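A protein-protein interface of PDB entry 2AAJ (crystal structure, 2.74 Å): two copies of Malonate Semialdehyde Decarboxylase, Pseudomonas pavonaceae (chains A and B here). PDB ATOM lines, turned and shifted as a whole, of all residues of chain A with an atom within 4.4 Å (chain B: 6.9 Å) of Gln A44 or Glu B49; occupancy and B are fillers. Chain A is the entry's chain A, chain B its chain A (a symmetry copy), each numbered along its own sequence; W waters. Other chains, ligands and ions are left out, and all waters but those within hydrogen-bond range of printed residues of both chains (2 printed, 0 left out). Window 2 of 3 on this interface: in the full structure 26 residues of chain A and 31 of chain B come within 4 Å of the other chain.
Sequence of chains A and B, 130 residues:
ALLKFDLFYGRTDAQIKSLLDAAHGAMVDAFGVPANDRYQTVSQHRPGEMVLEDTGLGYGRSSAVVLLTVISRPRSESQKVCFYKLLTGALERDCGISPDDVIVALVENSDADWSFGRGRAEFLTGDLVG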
ATOM      1  N   LEU A   7      16.270 -12.838  29.624  1.00  0.00           N
ATOM      2  CA  LEU A   7      15.941 -13.261  30.984  1.00  0.00           C
ATOM      3  C   LEU A   7      16.025 -14.789  31.014  1.00  0.00           C
ATOM      4  O   LEU A   7      16.081 -15.407  29.963  1.00  0.00           O
ATOM      5  CB  LEU A   7      14.579 -12.666  31.454  1.00  0.00           C
ATOM      6  CG  LEU A   7      13.340 -13.489  31.030  1.00  0.00           C
ATOM      7  CD1 LEU A   7      11.960 -12.991  31.376  1.00  0.00           C
ATOM      8  CD2 LEU A   7      13.288 -13.585  29.601  1.00  0.00           C
ATOM      9  N   PHE A   8      16.121 -15.405  32.198  1.00  0.00           N
ATOM     10  CA  PHE A   8      16.225 -16.874  32.340  1.00  0.00           C
ATOM     11  C   PHE A   8      14.820 -17.415  32.481  1.00  0.00           C
ATOM     12  O   PHE A   8      13.949 -16.715  32.983  1.00  0.00           O
ATOM     13  CB  PHE A   8      17.007 -17.252  33.600  1.00  0.00           C
ATOM     14  CG  PHE A   8      18.515 -17.224  33.445  1.00  0.00           C
ATOM     15  CD1 PHE A   8      19.182 -18.040  32.488  1.00  0.00           C
ATOM     16  CD2 PHE A   8      19.290 -16.441  34.308  1.00  0.00           C
ATOM     17  CE1 PHE A   8      20.626 -18.011  32.376  1.00  0.00           C
ATOM     18  CE2 PHE A   8      20.680 -16.394  34.207  1.00  0.00           C
ATOM     19  CZ  PHE A   8      21.360 -17.182  33.259  1.00  0.00           C
ATOM     20  N   TYR A   9      14.582 -18.658  32.074  1.00  0.00           N
ATOM     21  CA  TYR A   9      13.256 -19.268  32.264  1.00  0.00           C
ATOM     22  C   TYR A   9      12.932 -19.310  33.747  1.00  0.00           C
ATOM     23  O   TYR A   9      13.819 -19.543  34.560  1.00  0.00           O
ATOM     24  CB  TYR A   9      13.209 -20.686  31.703  1.00  0.00           C
ATOM     25  CG  TYR A   9      13.002 -20.813  30.202  1.00  0.00           C
ATOM     26  CD1 TYR A   9      11.773 -20.510  29.613  1.00  0.00           C
ATOM     27  CD2 TYR A   9      14.044 -21.271  29.364  1.00  0.00           C
ATOM     28  CE1 TYR A   9      11.581 -20.665  28.214  1.00  0.00           C
ATOM     29  CE2 TYR A   9      13.861 -21.429  27.988  1.00  0.00           C
ATOM     30  CZ  TYR A   9      12.628 -21.120  27.413  1.00  0.00           C
ATOM     31  OH  TYR A   9      12.471 -21.272  26.050  1.00  0.00           O
ATOM     32  N   GLY A  10      11.672 -19.098  34.107  1.00  0.00           N
ATOM     33  CA  GLY A  10      11.280 -19.218  35.496  1.00  0.00           C
ATOM     34  C   GLY A  10      10.023 -18.416  35.820  1.00  0.00           C
ATOM     35  O   GLY A  10       9.201 -18.845  36.656  1.00  0.00           O
ATOM     36  N   ILE A  16       6.258 -11.706  33.626  1.00  0.00           N
ATOM     37  CA  ILE A  16       6.888 -11.095  32.447  1.00  0.00           C
ATOM     38  C   ILE A  16       6.225  -9.758  32.115  1.00  0.00           C
ATOM     39  O   ILE A  16       6.929  -8.787  31.859  1.00  0.00           O
ATOM     40  CB  ILE A  16       6.942 -12.097  31.226  1.00  0.00           C
ATOM     41  CG1 ILE A  16       7.875 -13.279  31.540  1.00  0.00           C
ATOM     42  CG2 ILE A  16       7.414 -11.414  29.954  1.00  0.00           C
ATOM     43  CD1 ILE A  16       7.944 -14.341  30.425  1.00  0.00           C
ATOM     44  N   GLN A  40       8.788  -3.738  22.480  1.00  0.00           N
ATOM     45  CA  GLN A  40       9.451  -4.612  23.411  1.00  0.00           C
ATOM     46  C   GLN A  40       9.480  -6.093  22.989  1.00  0.00           C
ATOM     47  O   GLN A  40       8.481  -6.605  22.485  1.00  0.00           O
ATOM     48  CB  GLN A  40       8.803  -4.516  24.783  1.00  0.00           C
ATOM     49  CG  GLN A  40       8.694  -3.131  25.376  1.00  0.00           C
ATOM     50  CD  GLN A  40       8.018  -3.160  26.744  1.00  0.00           C
ATOM     51  OE1 GLN A  40       6.885  -3.647  26.870  1.00  0.00           O
ATOM     52  NE2 GLN A  40       8.711  -2.661  27.770  1.00  0.00           N
ATOM     53  N   THR A  41      10.610  -6.772  23.243  1.00  0.00           N
ATOM     54  CA  THR A  41      10.770  -8.208  22.964  1.00  0.00           C
ATOM     55  C   THR A  41      11.355  -8.924  24.209  1.00  0.00           C
ATOM     56  O   THR A  41      12.009  -8.278  25.045  1.00  0.00           O
ATOM     57  CB  THR A  41      11.690  -8.508  21.688  1.00  0.00           C
ATOM     58  OG1 THR A  41      13.073  -8.146  21.937  1.00  0.00           O
ATOM     59  CG2 THR A  41      11.286  -7.714  20.422  1.00  0.00           C
ATOM     60  N   VAL A  42      11.132 -10.244  24.323  1.00  0.00           N
ATOM     61  CA  VAL A  42      11.653 -11.039  25.450  1.00  0.00           C
ATOM     62  C   VAL A  42      12.171 -12.377  24.945  1.00  0.00           C
ATOM     63  O   VAL A  42      11.462 -13.069  24.279  1.00  0.00           O
ATOM     64  CB  VAL A  42      10.529 -11.392  26.507  1.00  0.00           C
ATOM     65  CG1 VAL A  42      11.045 -11.857  27.699  1.00  0.00           C
ATOM     66  CG2 VAL A  42       9.884 -10.277  26.986  1.00  0.00           C
ATOM     67  N   SER A  43      13.406 -12.725  25.275  1.00  0.00           N
ATOM     68  CA  SER A  43      13.921 -14.059  25.036  1.00  0.00           C
ATOM     69  C   SER A  43      14.252 -14.665  26.368  1.00  0.00           C
ATOM     70  O   SER A  43      14.915 -14.045  27.210  1.00  0.00           O
ATOM     71  CB  SER A  43      15.151 -14.048  24.151  1.00  0.00           C
ATOM     72  OG  SER A  43      14.883 -13.095  23.150  1.00  0.00           O
ATOM     73  N   GLN A  44      13.760 -15.874  26.545  1.00  0.00           N
ATOM     74  CA  GLN A  44      14.031 -16.645  27.702  1.00  0.00           C
ATOM     75  C   GLN A  44      15.141 -17.693  27.443  1.00  0.00           C
ATOM     76  O   GLN A  44      15.131 -18.389  26.433  1.00  0.00           O
ATOM     77  CB  GLN A  44      12.741 -17.321  28.115  1.00  0.00           C
ATOM     78  CG  GLN A  44      11.554 -16.351  28.286  1.00  0.00           C
ATOM     79  CD  GLN A  44      10.483 -16.901  29.204  1.00  0.00           C
ATOM     80  OE1 GLN A  44      10.769 -17.297  30.333  1.00  0.00           O
ATOM     81  NE2 GLN A  44       9.256 -16.951  28.712  1.00  0.00           N
ATOM     82  N   HIS A  45      16.074 -17.810  28.386  1.00  0.00           N
ATOM     83  CA  HIS A  45      17.207 -18.687  28.249  1.00  0.00           C
ATOM     84  C   HIS A  45      17.202 -19.778  29.339  1.00  0.00           C
ATOM     85  O   HIS A  45      16.695 -19.567  30.443  1.00  0.00           O
ATOM     86  CB  HIS A  45      18.484 -17.829  28.317  1.00  0.00           C
ATOM     87  CG  HIS A  45      18.616 -16.853  27.181  1.00  0.00           C
ATOM     88  ND1 HIS A  45      18.063 -15.588  27.208  1.00  0.00           N
ATOM     89  CD2 HIS A  45      19.203 -16.971  25.973  1.00  0.00           C
ATOM     90  CE1 HIS A  45      18.302 -14.969  26.075  1.00  0.00           C
ATOM     91  NE2 HIS A  45      19.018 -15.781  25.318  1.00  0.00           N
ATOM     92  N   PHE B   8       6.010 -13.526  15.733  1.00  0.00           N
ATOM     93  CA  PHE B   8       5.217 -14.338  16.681  1.00  0.00           C
ATOM     94  C   PHE B   8       5.100 -15.728  16.099  1.00  0.00           C
ATOM     95  O   PHE B   8       5.120 -15.879  14.883  1.00  0.00           O
ATOM     96  CB  PHE B   8       3.805 -13.773  16.845  1.00  0.00           C
ATOM     97  CG  PHE B   8       3.689 -12.625  17.829  1.00  0.00           C
ATOM     98  CD1 PHE B   8       4.054 -12.777  19.198  1.00  0.00           C
ATOM     99  CD2 PHE B   8       3.140 -11.406  17.418  1.00  0.00           C
ATOM    100  CE1 PHE B   8       3.911 -11.670  20.123  1.00  0.00           C
ATOM    101  CE2 PHE B   8       3.006 -10.329  18.292  1.00  0.00           C
ATOM    102  CZ  PHE B   8       3.372 -10.450  19.647  1.00  0.00           C
ATOM    103  N   TYR B   9       4.950 -16.750  16.936  1.00  0.00           N
ATOM    104  CA  TYR B   9       4.747 -18.115  16.424  1.00  0.00           C
ATOM    105  C   TYR B   9       3.480 -18.152  15.587  1.00  0.00           C
ATOM    106  O   TYR B   9       2.506 -17.487  15.923  1.00  0.00           O
ATOM    107  CB  TYR B   9       4.621 -19.124  17.562  1.00  0.00           C
ATOM    108  CG  TYR B   9       5.922 -19.602  18.187  1.00  0.00           C
ATOM    109  CD1 TYR B   9       6.789 -20.449  17.496  1.00  0.00           C
ATOM    110  CD2 TYR B   9       6.275 -19.224  19.503  1.00  0.00           C
ATOM    111  CE1 TYR B   9       7.986 -20.917  18.103  1.00  0.00           C
ATOM    112  CE2 TYR B   9       7.447 -19.683  20.108  1.00  0.00           C
ATOM    113  CZ  TYR B   9       8.306 -20.526  19.403  1.00  0.00           C
ATOM    114  OH  TYR B   9       9.466 -20.961  20.013  1.00  0.00           O
ATOM    115  N   GLN B  44      11.189 -16.532  17.104  1.00  0.00           N
ATOM    116  CA  GLN B  44       9.783 -16.619  17.252  1.00  0.00           C
ATOM    117  C   GLN B  44       9.353 -16.463  18.731  1.00  0.00           C
ATOM    118  O   GLN B  44       9.936 -17.066  19.627  1.00  0.00           O
ATOM    119  CB  GLN B  44       9.347 -17.962  16.705  1.00  0.00           C
ATOM    120  CG  GLN B  44       9.833 -18.240  15.268  1.00  0.00           C
ATOM    121  CD  GLN B  44       8.971 -19.255  14.550  1.00  0.00           C
ATOM    122  OE1 GLN B  44       7.752 -19.102  14.477  1.00  0.00           O
ATOM    123  NE2 GLN B  44       9.595 -20.305  14.043  1.00  0.00           N
ATOM    124  N   HIS B  45       8.308 -15.671  18.962  1.00  0.00           N
ATOM    125  CA  HIS B  45       7.843 -15.371  20.290  1.00  0.00           C
ATOM    126  C   HIS B  45       6.403 -15.879  20.504  1.00  0.00           C
ATOM    127  O   HIS B  45       5.613 -15.960  19.560  1.00  0.00           O
ATOM    128  CB  HIS B  45       7.938 -13.848  20.497  1.00  0.00           C
ATOM    129  CG  HIS B  45       9.347 -13.321  20.456  1.00  0.00           C
ATOM    130  ND1 HIS B  45       9.978 -12.952  19.285  1.00  0.00           N
ATOM    131  CD2 HIS B  45      10.254 -13.139  21.437  1.00  0.00           C
ATOM    132  CE1 HIS B  45      11.207 -12.565  19.541  1.00  0.00           C
ATOM    133  NE2 HIS B  45      11.389 -12.645  20.846  1.00  0.00           N
ATOM    134  N   ARG B  46       6.058 -16.235  21.740  1.00  0.00           N
ATOM    135  CA  ARG B  46       4.645 -16.433  22.101  1.00  0.00           C
ATOM    136  C   ARG B  46       3.961 -15.053  22.409  1.00  0.00           C
ATOM    137  O   ARG B  46       4.659 -14.018  22.540  1.00  0.00           O
ATOM    138  CB  ARG B  46       4.551 -17.353  23.291  1.00  0.00           C
ATOM    139  CG  ARG B  46       5.154 -18.728  23.127  1.00  0.00           C
ATOM    140  CD  ARG B  46       5.409 -19.388  24.465  1.00  0.00           C
ATOM    141  NE  ARG B  46       4.716 -18.608  25.503  1.00  0.00           N
ATOM    142  CZ  ARG B  46       5.309 -17.947  26.500  1.00  0.00           C
ATOM    143  NH1 ARG B  46       6.626 -17.973  26.677  1.00  0.00           N
ATOM    144  NH2 ARG B  46       4.572 -17.250  27.318  1.00  0.00           N
ATOM    145  N   PRO B  47       2.631 -14.990  22.528  1.00  0.00           N
ATOM    146  CA  PRO B  47       1.986 -13.682  22.796  1.00  0.00           C
ATOM    147  C   PRO B  47       2.531 -12.935  24.043  1.00  0.00           C
ATOM    148  O   PRO B  47       2.689 -11.697  24.012  1.00  0.00           O
ATOM    149  CB  PRO B  47       0.492 -14.018  22.860  1.00  0.00           C
ATOM    150  CG  PRO B  47       0.416 -15.248  21.983  1.00  0.00           C
ATOM    151  CD  PRO B  47       1.648 -16.070  22.353  1.00  0.00           C
ATOM    152  N   GLY B  48       2.875 -13.650  25.108  1.00  0.00           N
ATOM    153  CA  GLY B  48       3.666 -13.003  26.147  1.00  0.00           C
ATOM    154  C   GLY B  48       4.822 -12.070  25.664  1.00  0.00           C
ATOM    155  O   GLY B  48       5.019 -10.958  26.219  1.00  0.00           O
ATOM    156  N   GLU B  49       5.561 -12.463  24.615  1.00  0.00           N
ATOM    157  CA  GLU B  49       6.972 -12.084  24.552  1.00  0.00           C
ATOM    158  C   GLU B  49       7.385 -10.981  23.609  1.00  0.00           C
ATOM    159  O   GLU B  49       8.585 -10.764  23.410  1.00  0.00           O
ATOM    160  CB  GLU B  49       7.833 -13.329  24.344  1.00  0.00           C
ATOM    161  CG  GLU B  49       7.543 -14.485  25.299  1.00  0.00           C
ATOM    162  CD  GLU B  49       8.295 -15.749  24.940  1.00  0.00           C
ATOM    163  OE1 GLU B  49       8.263 -16.179  23.771  1.00  0.00           O
ATOM    164  OE2 GLU B  49       8.912 -16.328  25.837  1.00  0.00           O
ATOM    165  N   MET B  50       6.400 -10.302  23.037  1.00  0.00           N
ATOM    166  CA  MET B  50       6.618  -9.052  22.317  1.00  0.00           C
ATOM    167  C   MET B  50       5.425  -8.158  22.581  1.00  0.00           C
ATOM    168  O   MET B  50       4.278  -8.638  22.611  1.00  0.00           O
ATOM    169  CB  MET B  50       6.633  -9.240  20.803  1.00  0.00           C
ATOM    170  CG  MET B  50       7.664 -10.126  20.215  1.00  0.00           C
ATOM    171  SD  MET B  50       8.102  -9.586  18.550  1.00  0.00           S
ATOM    172  CE  MET B  50       6.758 -10.143  17.597  1.00  0.00           C
ATOM    173  N   VAL B  51       5.680  -6.859  22.744  1.00  0.00           N
ATOM    174  CA  VAL B  51       4.615  -5.855  22.765  1.00  0.00           C
ATOM    175  C   VAL B  51       5.055  -4.831  21.768  1.00  0.00           C
ATOM    176  O   VAL B  51       6.121  -4.266  21.902  1.00  0.00           O
ATOM    177  CB  VAL B  51       4.373  -5.223  24.158  1.00  0.00           C
ATOM    178  CG1 VAL B  51       3.251  -4.177  24.084  1.00  0.00           C
ATOM    179  CG2 VAL B  51       4.101  -6.324  25.205  1.00  0.00           C
HETATM  180  O   HOH W   1      12.121 -16.678  24.490  1.00  0.00           O
HETATM  181  O   HOH W   2      14.031 -11.398  21.374  1.00  0.00           O
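The backbone NH (N) of Gln A40 lies within hydrogen-bond range of the backbone carbonyl oxygen (O) of Val B51, 2.8 Å away. O of Val A42 sits close to NE2 of His B45, 3.5 Å away. O of Glu B49 is in hydrogen-bond range of N of Val A42 (2.8 Å). The guanidinium group of Arg B46 lies close to the side-chain amide nitrogen of Gln A44. The side-chain amide nitrogen (NE2) of Gln A44 lies within hydrogen-bond range of the side-chain carboxylate (OE2) of Glu B49 (3.0 Å).
The backbone carbonyl oxygen of His B45 is in hydrogen-bond range of the backbone NH of Tyr B9, 2.8 Å away. The guanidinium group (NH1) of Arg B46 lies within salt-bridge range of the side-chain carboxylate (OE2) of Glu B49.
CA of Met B50 touches O of Gln A40 (3.1 Å). Thr A41 touches Glu B49.
Printed residues of chain B within 4 Å of Thr A41: Glu B49. Printed residues of chain A within 4 Å of Arg B46: Gln A44. Gly B48 touches none of the printed residues of chain A. Of the printed residues of chain A, Glu B49 touches Thr A41 (3.4 Å), Val A42 (2.8 Å) and Gln A44 (3.0 Å). Of the printed residues of chain A, Val B51 touches Gln A40 (2.8 Å). The nearest printed residue of chain A that does not touch Val B51 is Thr A41 (5.0 Å).
Hydrophobic or aromatic side chains of chain A that line the printed part of chain B: Val A42. Hydrophobic or aromatic side chains of chain B within 4 Å of the printed part of chain A: His B45 and Met B50. Among the printed residues, 7 pairs touch across the chains. Among the printed residues, no Asp or Glu carboxylate lies within 4 Å of a Lys or Arg side-chain nitrogen of the other chain.
Positions printed for both chains: 8, 9, 44 and 45. Of the 7 pairs that touch across the chains among the printed residues, none has its exchanged pair printed and touching as well.
Water W2 lies within hydrogen-bond range of OG of Ser A43, NE2 of His B45 and OG1 of Thr A41. Water W1 bridges N of Gln A44 and OE2 of Glu B49.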
